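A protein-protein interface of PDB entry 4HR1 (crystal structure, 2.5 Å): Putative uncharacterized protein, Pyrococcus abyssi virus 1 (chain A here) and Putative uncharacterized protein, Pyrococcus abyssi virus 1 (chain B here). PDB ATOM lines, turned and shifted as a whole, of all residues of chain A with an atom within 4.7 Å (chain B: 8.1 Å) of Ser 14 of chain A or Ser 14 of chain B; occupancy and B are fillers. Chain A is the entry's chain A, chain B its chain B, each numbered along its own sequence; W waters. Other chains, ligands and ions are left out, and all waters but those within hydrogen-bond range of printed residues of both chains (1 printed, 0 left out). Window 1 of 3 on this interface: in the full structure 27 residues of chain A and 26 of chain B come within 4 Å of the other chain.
Of the printed residues of chain B, Gln 11 of chain A touches Leu 118, Asp 119 and Ser 120. Ser 14 of chain A touches just one residue of chain B: Ser 14. Ser 14 of chain B touches just one residue of chain A: Ser 14. Val 47 of chain B touches none of the printed residues of chain A. Printed residues of chain A within 4 Å of Ser 120 of chain B: Gln 11. The nearest printed residue of chain A that does not touch Ser 14 of chain B is Thr 18 of chain A (5.3 Å). The nearest printed residue of chain A that does not touch Thr 18 of chain B is Ser 14 of chain A (5.4 Å).
Among the printed residues, pairs that only touch across the chains: Ile 10 of chain A with Thr 18 of chain B, Ile 10 of chain A with Leu 118 of chain B, Ile 10 of chain A with Asp 119 of chain B, Gln 11 of chain A with Ser 120 of chain B, Ser 14 of chain A with Ser 14 of chain B, Arg 17 of chain A with Arg 17 of chain B and Thr 18 of chain A with Ile 10 of chain B.
Water W1 lies within hydrogen-bond range of the side-chain amide nitrogen of Gln 11 of chain B, the backbone carbonyl oxygen of Asp 119 of chain B and the backbone carbonyl oxygen of Asp 119 of chain A.
The backbone NH of Trp 15 of chain A is in hydrogen-bond range of the side-chain carboxylate of Asp 119 of chain A, 3.2 Å away. O of Ser 14 of chain B lies within hydrogen-bond range of OG1 of Thr 18 of chain B (2.8 Å). OE1 of Gln 11 of chain B sits close to O of Asp 119 of chain B (3.4 Å). The side-chain hydroxyl of Ser 14 of chain A sits at hydrogen-bond distance from the backbone carbonyl oxygen of Ile 10 of chain A. OG of Ser 14 of chain B lies within hydrogen-bond range of O of Ile 10 of chain B, at 2.8 Å. The side-chain hydroxyl (OG1) of Thr 18 of chain B is in hydrogen-bond range of the side-chain carboxylate (OD1) of Asp 119 of chain B, at 3.3 Å.
The backbone carbonyl oxygen (O) of Leu 118 of chain B lies within hydrogen-bond range of the side-chain amide nitrogen (NE2) of Gln 11 of chain A (2.8 Å). The backbone carbonyl oxygen (O) of Asp 119 of chain A lies close to the side-chain amide oxygen (OE1) of Gln 11 of chain B (3.3 Å). The side-chain amide nitrogen (NE2) of Gln 11 of chain A sits at hydrogen-bond distance from the backbone carbonyl oxygen (O) of Asp 119 of chain B, at 3.2 Å. The backbone carbonyl oxygen (O) of Asp 119 of chain A sits close to the backbone carbonyl oxygen (O) of Asp 119 of chain B.
Of the 22 printed residues of chain B, 8 touch a printed residue of chain A. Printed residues of chain B that touch a printed residue of chain A: Ile 10, Gln 11, Ser 14, Arg 17, Thr 18, Leu 118, Asp 119 and Ser 120. Hydrophobic or aromatic side chains of chain B within 4 Å of the printed part of chain A: Ile 10.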
ATOM      1  N   ILE A  10     -18.672 -23.709  30.594  1.00  0.00           N
ATOM      2  CA  ILE A  10     -19.557 -22.599  30.244  1.00  0.00           C
ATOM      3  C   ILE A  10     -20.702 -22.478  31.253  1.00  0.00           C
ATOM      4  O   ILE A  10     -20.902 -21.391  31.801  1.00  0.00           O
ATOM      5  CB  ILE A  10     -20.012 -22.649  28.736  1.00  0.00           C
ATOM      6  CG1 ILE A  10     -18.822 -22.338  27.758  1.00  0.00           C
ATOM      7  CG2 ILE A  10     -21.199 -21.700  28.464  1.00  0.00           C
ATOM      8  CD1 ILE A  10     -17.875 -21.024  28.213  1.00  0.00           C
ATOM      9  N   GLN A  11     -21.381 -23.601  31.575  1.00  0.00           N
ATOM     10  CA  GLN A  11     -22.469 -23.605  32.557  1.00  0.00           C
ATOM     11  C   GLN A  11     -22.016 -23.133  33.936  1.00  0.00           C
ATOM     12  O   GLN A  11     -22.723 -22.348  34.587  1.00  0.00           O
ATOM     13  CB  GLN A  11     -23.130 -24.991  32.652  1.00  0.00           C
ATOM     14  CG  GLN A  11     -23.906 -25.446  31.398  1.00  0.00           C
ATOM     15  CD  GLN A  11     -24.908 -24.434  30.882  1.00  0.00           C
ATOM     16  OE1 GLN A  11     -25.774 -23.926  31.613  1.00  0.00           O
ATOM     17  NE2 GLN A  11     -24.798 -24.117  29.602  1.00  0.00           N
ATOM     18  N   LYS A  12     -20.820 -23.564  34.356  1.00  0.00           N
ATOM     19  CA  LYS A  12     -20.258 -23.189  35.648  1.00  0.00           C
ATOM     20  C   LYS A  12     -19.890 -21.704  35.688  1.00  0.00           C
ATOM     21  O   LYS A  12     -20.177 -21.028  36.690  1.00  0.00           O
ATOM     22  CB  LYS A  12     -19.046 -24.096  36.015  1.00  0.00           C
ATOM     23  CG  LYS A  12     -19.388 -25.587  36.264  1.00  0.00           C
ATOM     24  CD  LYS A  12     -19.612 -25.910  37.754  1.00  0.00           C
ATOM     25  CE  LYS A  12     -20.574 -27.063  37.992  1.00  0.00           C
ATOM     26  NZ  LYS A  12     -21.105 -27.079  39.395  1.00  0.00           N
ATOM     27  N   ILE A  13     -19.267 -21.183  34.595  1.00  0.00           N
ATOM     28  CA  ILE A  13     -18.889 -19.759  34.508  1.00  0.00           C
ATOM     29  C   ILE A  13     -20.186 -18.912  34.472  1.00  0.00           C
ATOM     30  O   ILE A  13     -20.315 -17.968  35.258  1.00  0.00           O
ATOM     31  CB  ILE A  13     -17.900 -19.452  33.318  1.00  0.00           C
ATOM     32  CG1 ILE A  13     -16.553 -20.230  33.459  1.00  0.00           C
ATOM     33  CG2 ILE A  13     -17.629 -17.934  33.201  1.00  0.00           C
ATOM     34  CD1 ILE A  13     -15.774 -20.539  32.073  1.00  0.00           C
ATOM     35  N   SER A  14     -21.159 -19.294  33.608  1.00  0.00           N
ATOM     36  CA  SER A  14     -22.456 -18.599  33.507  1.00  0.00           C
ATOM     37  C   SER A  14     -23.161 -18.510  34.860  1.00  0.00           C
ATOM     38  O   SER A  14     -23.527 -17.402  35.252  1.00  0.00           O
ATOM     39  CB  SER A  14     -23.363 -19.242  32.461  1.00  0.00           C
ATOM     40  OG  SER A  14     -22.749 -19.226  31.180  1.00  0.00           O
ATOM     41  N   TRP A  15     -23.268 -19.645  35.613  1.00  0.00           N
ATOM     42  CA  TRP A  15     -23.876 -19.654  36.952  1.00  0.00           C
ATOM     43  C   TRP A  15     -23.173 -18.661  37.832  1.00  0.00           C
ATOM     44  O   TRP A  15     -23.827 -17.845  38.488  1.00  0.00           O
ATOM     45  CB  TRP A  15     -23.779 -21.048  37.626  1.00  0.00           C
ATOM     46  CG  TRP A  15     -24.696 -21.209  38.806  1.00  0.00           C
ATOM     47  CD1 TRP A  15     -25.963 -21.718  38.783  1.00  0.00           C
ATOM     48  CD2 TRP A  15     -24.469 -20.762  40.154  1.00  0.00           C
ATOM     49  NE1 TRP A  15     -26.514 -21.676  40.041  1.00  0.00           N
ATOM     50  CE2 TRP A  15     -25.623 -21.088  40.903  1.00  0.00           C
ATOM     51  CE3 TRP A  15     -23.370 -20.182  40.826  1.00  0.00           C
ATOM     52  CZ2 TRP A  15     -25.724 -20.837  42.279  1.00  0.00           C
ATOM     53  CZ3 TRP A  15     -23.487 -19.904  42.181  1.00  0.00           C
ATOM     54  CH2 TRP A  15     -24.658 -20.213  42.889  1.00  0.00           C
ATOM     55  N   LEU A  16     -21.839 -18.743  37.872  1.00  0.00           N
ATOM     56  CA  LEU A  16     -21.024 -17.870  38.727  1.00  0.00           C
ATOM     57  C   LEU A  16     -21.162 -16.380  38.375  1.00  0.00           C
ATOM     58  O   LEU A  16     -21.259 -15.556  39.291  1.00  0.00           O
ATOM     59  CB  LEU A  16     -19.560 -18.325  38.729  1.00  0.00           C
ATOM     60  CG  LEU A  16     -19.262 -19.640  39.458  1.00  0.00           C
ATOM     61  CD1 LEU A  16     -17.842 -20.020  39.292  1.00  0.00           C
ATOM     62  CD2 LEU A  16     -19.535 -19.532  40.931  1.00  0.00           C
ATOM     63  N   ARG A  17     -21.255 -16.044  37.060  1.00  0.00           N
ATOM     64  CA  ARG A  17     -21.436 -14.654  36.617  1.00  0.00           C
ATOM     65  C   ARG A  17     -22.817 -14.126  37.022  1.00  0.00           C
ATOM     66  O   ARG A  17     -22.909 -13.045  37.624  1.00  0.00           O
ATOM     67  CB  ARG A  17     -21.174 -14.487  35.112  1.00  0.00           C
ATOM     68  CG  ARG A  17     -19.710 -14.726  34.738  1.00  0.00           C
ATOM     69  CD  ARG A  17     -19.236 -13.769  33.670  1.00  0.00           C
ATOM     70  NE  ARG A  17     -18.375 -14.420  32.676  1.00  0.00           N
ATOM     71  CZ  ARG A  17     -17.045 -14.424  32.716  1.00  0.00           C
ATOM     72  NH1 ARG A  17     -16.400 -13.841  33.723  1.00  0.00           N
ATOM     73  NH2 ARG A  17     -16.351 -15.027  31.764  1.00  0.00           N
ATOM     74  N   THR A  18     -23.873 -14.934  36.774  1.00  0.00           N
ATOM     75  CA  THR A  18     -25.264 -14.634  37.125  1.00  0.00           C
ATOM     76  C   THR A  18     -25.402 -14.469  38.645  1.00  0.00           C
ATOM     77  O   THR A  18     -26.137 -13.580  39.100  1.00  0.00           O
ATOM     78  CB  THR A  18     -26.207 -15.700  36.565  1.00  0.00           C
ATOM     79  OG1 THR A  18     -25.826 -16.080  35.229  1.00  0.00           O
ATOM     80  CG2 THR A  18     -27.670 -15.268  36.613  1.00  0.00           C
ATOM     81  N   ASP A 119     -29.988 -20.014  33.608  1.00  0.00           N
ATOM     82  CA  ASP A 119     -28.933 -20.690  32.835  1.00  0.00           C
ATOM     83  C   ASP A 119     -29.392 -21.714  31.803  1.00  0.00           C
ATOM     84  O   ASP A 119     -28.665 -21.967  30.837  1.00  0.00           O
ATOM     85  CB  ASP A 119     -27.973 -21.384  33.809  1.00  0.00           C
ATOM     86  CG  ASP A 119     -26.719 -20.598  34.082  1.00  0.00           C
ATOM     87  OD1 ASP A 119     -26.827 -19.368  34.320  1.00  0.00           O
ATOM     88  OD2 ASP A 119     -25.626 -21.211  34.070  1.00  0.00           O
ATOM     89  N   GLN B   7     -33.931 -14.159  32.297  1.00  0.00           N
ATOM     90  CA  GLN B   7     -33.507 -15.316  31.502  1.00  0.00           C
ATOM     91  C   GLN B   7     -33.040 -14.893  30.112  1.00  0.00           C
ATOM     92  O   GLN B   7     -31.979 -15.347  29.692  1.00  0.00           O
ATOM     93  CB  GLN B   7     -34.599 -16.399  31.426  1.00  0.00           C
ATOM     94  CG  GLN B   7     -34.133 -17.711  30.798  1.00  0.00           C
ATOM     95  CD  GLN B   7     -35.029 -18.144  29.665  1.00  0.00           C
ATOM     96  OE1 GLN B   7     -35.964 -18.926  29.852  1.00  0.00           O
ATOM     97  NE2 GLN B   7     -34.762 -17.655  28.456  1.00  0.00           N
ATOM     98  N   THR B   8     -33.813 -14.005  29.421  1.00  0.00           N
ATOM     99  CA  THR B   8     -33.497 -13.484  28.086  1.00  0.00           C
ATOM    100  C   THR B   8     -32.133 -12.757  28.072  1.00  0.00           C
ATOM    101  O   THR B   8     -31.288 -13.059  27.224  1.00  0.00           O
ATOM    102  CB  THR B   8     -34.669 -12.631  27.539  1.00  0.00           C
ATOM    103  OG1 THR B   8     -35.765 -13.495  27.224  1.00  0.00           O
ATOM    104  CG2 THR B   8     -34.297 -11.876  26.271  1.00  0.00           C
ATOM    105  N   VAL B   9     -31.936 -11.830  29.037  1.00  0.00           N
ATOM    106  CA  VAL B   9     -30.715 -11.044  29.218  1.00  0.00           C
ATOM    107  C   VAL B   9     -29.481 -11.904  29.506  1.00  0.00           C
ATOM    108  O   VAL B   9     -28.454 -11.686  28.867  1.00  0.00           O
ATOM    109  CB  VAL B   9     -30.858  -9.806  30.165  1.00  0.00           C
ATOM    110  CG1 VAL B   9     -32.218  -9.137  30.010  1.00  0.00           C
ATOM    111  CG2 VAL B   9     -30.597 -10.156  31.628  1.00  0.00           C
ATOM    112  N   ILE B  10     -29.597 -12.890  30.439  1.00  0.00           N
ATOM    113  CA  ILE B  10     -28.515 -13.808  30.800  1.00  0.00           C
ATOM    114  C   ILE B  10     -28.157 -14.662  29.587  1.00  0.00           C
ATOM    115  O   ILE B  10     -26.974 -14.768  29.244  1.00  0.00           O
ATOM    116  CB  ILE B  10     -28.830 -14.643  32.093  1.00  0.00           C
ATOM    117  CG1 ILE B  10     -28.878 -13.759  33.374  1.00  0.00           C
ATOM    118  CG2 ILE B  10     -27.925 -15.896  32.275  1.00  0.00           C
ATOM    119  CD1 ILE B  10     -27.626 -12.861  33.716  1.00  0.00           C
ATOM    120  N   GLN B  11     -29.164 -15.219  28.909  1.00  0.00           N
ATOM    121  CA  GLN B  11     -28.899 -16.031  27.729  1.00  0.00           C
ATOM    122  C   GLN B  11     -28.208 -15.238  26.600  1.00  0.00           C
ATOM    123  O   GLN B  11     -27.352 -15.797  25.896  1.00  0.00           O
ATOM    124  CB  GLN B  11     -30.138 -16.825  27.262  1.00  0.00           C
ATOM    125  CG  GLN B  11     -30.626 -17.900  28.269  1.00  0.00           C
ATOM    126  CD  GLN B  11     -29.574 -18.865  28.817  1.00  0.00           C
ATOM    127  OE1 GLN B  11     -29.382 -19.976  28.308  1.00  0.00           O
ATOM    128  NE2 GLN B  11     -28.929 -18.502  29.922  1.00  0.00           N
ATOM    129  N   LYS B  12     -28.510 -13.921  26.503  1.00  0.00           N
ATOM    130  CA  LYS B  12     -27.902 -13.055  25.499  1.00  0.00           C
ATOM    131  C   LYS B  12     -26.471 -12.675  25.857  1.00  0.00           C
ATOM    132  O   LYS B  12     -25.599 -12.806  25.006  1.00  0.00           O
ATOM    133  CB  LYS B  12     -28.785 -11.833  25.166  1.00  0.00           C
ATOM    134  CG  LYS B  12     -29.846 -12.170  24.131  1.00  0.00           C
ATOM    135  CD  LYS B  12     -30.747 -10.989  23.815  1.00  0.00           C
ATOM    136  CE  LYS B  12     -31.987 -11.376  23.033  1.00  0.00           C
ATOM    137  NZ  LYS B  12     -31.681 -12.292  21.892  1.00  0.00           N
ATOM    138  N   ILE B  13     -26.227 -12.248  27.116  1.00  0.00           N
ATOM    139  CA  ILE B  13     -24.909 -11.889  27.636  1.00  0.00           C
ATOM    140  C   ILE B  13     -23.983 -13.121  27.612  1.00  0.00           C
ATOM    141  O   ILE B  13     -22.862 -13.004  27.130  1.00  0.00           O
ATOM    142  CB  ILE B  13     -25.035 -11.223  29.029  1.00  0.00           C
ATOM    143  CG1 ILE B  13     -25.814  -9.892  28.948  1.00  0.00           C
ATOM    144  CG2 ILE B  13     -23.661 -11.041  29.743  1.00  0.00           C
ATOM    145  CD1 ILE B  13     -26.137  -9.270  30.340  1.00  0.00           C
ATOM    146  N   SER B  14     -24.478 -14.306  28.038  1.00  0.00           N
ATOM    147  CA  SER B  14     -23.729 -15.572  28.027  1.00  0.00           C
ATOM    148  C   SER B  14     -23.287 -15.998  26.630  1.00  0.00           C
ATOM    149  O   SER B  14     -22.164 -16.483  26.477  1.00  0.00           O
ATOM    150  CB  SER B  14     -24.531 -16.711  28.670  1.00  0.00           C
ATOM    151  OG  SER B  14     -24.837 -16.464  30.033  1.00  0.00           O
ATOM    152  N   TRP B  15     -24.160 -15.863  25.625  1.00  0.00           N
ATOM    153  CA  TRP B  15     -23.825 -16.235  24.244  1.00  0.00           C
ATOM    154  C   TRP B  15     -22.674 -15.363  23.729  1.00  0.00           C
ATOM    155  O   TRP B  15     -21.717 -15.878  23.136  1.00  0.00           O
ATOM    156  CB  TRP B  15     -25.035 -16.092  23.319  1.00  0.00           C
ATOM    157  CG  TRP B  15     -24.826 -16.699  21.958  1.00  0.00           C
ATOM    158  CD1 TRP B  15     -25.269 -17.913  21.535  1.00  0.00           C
ATOM    159  CD2 TRP B  15     -24.093 -16.132  20.855  1.00  0.00           C
ATOM    160  NE1 TRP B  15     -24.892 -18.128  20.227  1.00  0.00           N
ATOM    161  CE2 TRP B  15     -24.198 -17.037  19.776  1.00  0.00           C
ATOM    162  CE3 TRP B  15     -23.453 -14.895  20.636  1.00  0.00           C
ATOM    163  CZ2 TRP B  15     -23.644 -16.773  18.516  1.00  0.00           C
ATOM    164  CZ3 TRP B  15     -22.891 -14.640  19.391  1.00  0.00           C
ATOM    165  CH2 TRP B  15     -22.968 -15.585  18.356  1.00  0.00           C
ATOM    166  N   LEU B  16     -22.785 -14.049  23.987  1.00  0.00           N
ATOM    167  CA  LEU B  16     -21.810 -13.042  23.594  1.00  0.00           C
ATOM    168  C   LEU B  16     -20.435 -13.357  24.247  1.00  0.00           C
ATOM    169  O   LEU B  16     -19.429 -13.403  23.542  1.00  0.00           O
ATOM    170  CB  LEU B  16     -22.307 -11.625  23.979  1.00  0.00           C
ATOM    171  CG  LEU B  16     -23.471 -11.023  23.187  1.00  0.00           C
ATOM    172  CD1 LEU B  16     -23.825  -9.672  23.728  1.00  0.00           C
ATOM    173  CD2 LEU B  16     -23.126 -10.838  21.746  1.00  0.00           C
ATOM    174  N   ARG B  17     -20.433 -13.642  25.566  1.00  0.00           N
ATOM    175  CA  ARG B  17     -19.234 -13.988  26.355  1.00  0.00           C
ATOM    176  C   ARG B  17     -18.545 -15.281  25.897  1.00  0.00           C
ATOM    177  O   ARG B  17     -17.320 -15.336  25.904  1.00  0.00           O
ATOM    178  CB  ARG B  17     -19.532 -14.034  27.853  1.00  0.00           C
ATOM    179  CG  ARG B  17     -19.899 -12.682  28.429  1.00  0.00           C
ATOM    180  CD  ARG B  17     -19.206 -12.449  29.731  1.00  0.00           C
ATOM    181  NE  ARG B  17     -20.117 -11.903  30.722  1.00  0.00           N
ATOM    182  CZ  ARG B  17     -20.104 -10.644  31.133  1.00  0.00           C
ATOM    183  NH1 ARG B  17     -19.240  -9.780  30.614  1.00  0.00           N
ATOM    184  NH2 ARG B  17     -20.952 -10.239  32.072  1.00  0.00           N
ATOM    185  N   THR B  18     -19.332 -16.269  25.450  1.00  0.00           N
ATOM    186  CA  THR B  18     -18.882 -17.565  24.935  1.00  0.00           C
ATOM    187  C   THR B  18     -18.302 -17.383  23.547  1.00  0.00           C
ATOM    188  O   THR B  18     -17.297 -18.015  23.231  1.00  0.00           O
ATOM    189  CB  THR B  18     -20.047 -18.599  24.968  1.00  0.00           C
ATOM    190  OG1 THR B  18     -20.499 -18.730  26.315  1.00  0.00           O
ATOM    191  CG2 THR B  18     -19.642 -19.976  24.458  1.00  0.00           C
ATOM    192  N   ALA B  19     -18.936 -16.526  22.708  1.00  0.00           N
ATOM    193  CA  ALA B  19     -18.456 -16.235  21.353  1.00  0.00           C
ATOM    194  C   ALA B  19     -17.078 -15.530  21.422  1.00  0.00           C
ATOM    195  O   ALA B  19     -16.177 -15.865  20.653  1.00  0.00           O
ATOM    196  CB  ALA B  19     -19.465 -15.384  20.612  1.00  0.00           C
ATOM    197  N   ILE B  20     -16.899 -14.633  22.398  1.00  0.00           N
ATOM    198  CA  ILE B  20     -15.640 -13.930  22.631  1.00  0.00           C
ATOM    199  C   ILE B  20     -14.556 -14.943  23.050  1.00  0.00           C
ATOM    200  O   ILE B  20     -13.420 -14.883  22.536  1.00  0.00           O
ATOM    201  CB  ILE B  20     -15.846 -12.789  23.656  1.00  0.00           C
ATOM    202  CG1 ILE B  20     -16.391 -11.548  22.945  1.00  0.00           C
ATOM    203  CG2 ILE B  20     -14.554 -12.459  24.419  1.00  0.00           C
ATOM    204  CD1 ILE B  20     -17.239 -10.687  23.788  1.00  0.00           C
ATOM    205  N   ALA B  21     -14.947 -15.908  23.949  1.00  0.00           N
ATOM    206  CA  ALA B  21     -14.102 -16.985  24.455  1.00  0.00           C
ATOM    207  C   ALA B  21     -13.694 -17.871  23.293  1.00  0.00           C
ATOM    208  O   ALA B  21     -12.540 -18.272  23.193  1.00  0.00           O
ATOM    209  CB  ALA B  21     -14.852 -17.795  25.506  1.00  0.00           C
ATOM    210  N   VAL B  47     -19.687  -5.842  25.754  1.00  0.00           N
ATOM    211  CA  VAL B  47     -20.462  -6.819  26.533  1.00  0.00           C
ATOM    212  C   VAL B  47     -20.428  -6.486  28.038  1.00  0.00           C
ATOM    213  O   VAL B  47     -21.481  -6.486  28.659  1.00  0.00           O
ATOM    214  CB  VAL B  47     -20.065  -8.281  26.243  1.00  0.00           C
ATOM    215  CG1 VAL B  47     -20.970  -9.261  26.988  1.00  0.00           C
ATOM    216  CG2 VAL B  47     -20.098  -8.563  24.747  1.00  0.00           C
ATOM    217  N   ALA B  51     -23.815  -5.337  30.185  1.00  0.00           N
ATOM    218  CA  ALA B  51     -24.073  -6.309  31.242  1.00  0.00           C
ATOM    219  C   ALA B  51     -24.337  -5.622  32.569  1.00  0.00           C
ATOM    220  O   ALA B  51     -25.371  -5.882  33.181  1.00  0.00           O
ATOM    221  CB  ALA B  51     -22.909  -7.275  31.377  1.00  0.00           C
ATOM    222  N   LEU B  85     -27.206  -5.182  22.554  1.00  0.00           N
ATOM    223  CA  LEU B  85     -26.779  -6.583  22.596  1.00  0.00           C
ATOM    224  C   LEU B  85     -26.902  -7.268  21.266  1.00  0.00           C
ATOM    225  O   LEU B  85     -26.068  -8.133  20.947  1.00  0.00           O
ATOM    226  CB  LEU B  85     -27.566  -7.385  23.652  1.00  0.00           C
ATOM    227  CG  LEU B  85     -27.276  -7.109  25.123  1.00  0.00           C
ATOM    228  CD1 LEU B  85     -28.273  -7.823  26.001  1.00  0.00           C
ATOM    229  CD2 LEU B  85     -25.892  -7.518  25.495  1.00  0.00           C
ATOM    230  N   LEU B 115     -22.390 -22.522  19.695  1.00  0.00           N
ATOM    231  CA  LEU B 115     -22.387 -21.625  20.849  1.00  0.00           C
ATOM    232  C   LEU B 115     -23.689 -21.733  21.631  1.00  0.00           C
ATOM    233  O   LEU B 115     -23.669 -21.678  22.868  1.00  0.00           O
ATOM    234  CB  LEU B 115     -22.073 -20.170  20.429  1.00  0.00           C
ATOM    235  CG  LEU B 115     -20.708 -19.939  19.732  1.00  0.00           C
ATOM    236  CD1 LEU B 115     -20.696 -18.635  18.970  1.00  0.00           C
ATOM    237  CD2 LEU B 115     -19.528 -20.028  20.714  1.00  0.00           C
ATOM    238  N   LEU B 118     -23.652 -24.833  23.812  1.00  0.00           N
ATOM    239  CA  LEU B 118     -22.817 -24.673  25.004  1.00  0.00           C
ATOM    240  C   LEU B 118     -23.554 -23.942  26.105  1.00  0.00           C
ATOM    241  O   LEU B 118     -23.269 -24.145  27.288  1.00  0.00           O
ATOM    242  CB  LEU B 118     -21.546 -23.894  24.628  1.00  0.00           C
ATOM    243  CG  LEU B 118     -20.256 -24.691  24.429  1.00  0.00           C
ATOM    244  CD1 LEU B 118     -20.448 -25.911  23.533  1.00  0.00           C
ATOM    245  CD2 LEU B 118     -19.189 -23.815  23.843  1.00  0.00           C
ATOM    246  N   ASP B 119     -24.488 -23.079  25.702  1.00  0.00           N
ATOM    247  CA  ASP B 119     -25.290 -22.211  26.558  1.00  0.00           C
ATOM    248  C   ASP B 119     -26.618 -22.801  27.045  1.00  0.00           C
ATOM    249  O   ASP B 119     -27.059 -22.446  28.143  1.00  0.00           O
ATOM    250  CB  ASP B 119     -25.559 -20.900  25.813  1.00  0.00           C
ATOM    251  CG  ASP B 119     -24.664 -19.756  26.223  1.00  0.00           C
ATOM    252  OD1 ASP B 119     -23.496 -20.010  26.599  1.00  0.00           O
ATOM    253  OD2 ASP B 119     -25.121 -18.607  26.150  1.00  0.00           O
ATOM    254  N   SER B 120     -27.270 -23.653  26.225  1.00  0.00           N
ATOM    255  CA  SER B 120     -28.566 -24.252  26.564  1.00  0.00           C
ATOM    256  C   SER B 120     -28.396 -25.572  27.301  1.00  0.00           C
ATOM    257  O   SER B 120     -27.825 -25.584  28.386  1.00  0.00           O
ATOM    258  CB  SER B 120     -29.443 -24.417  25.323  1.00  0.00           C
ATOM    259  OG  SER B 120     -28.894 -25.305  24.363  1.00  0.00           O
HETATM  260  O   HOH W   1     -26.141 -19.955  29.892  1.00  0.00           O
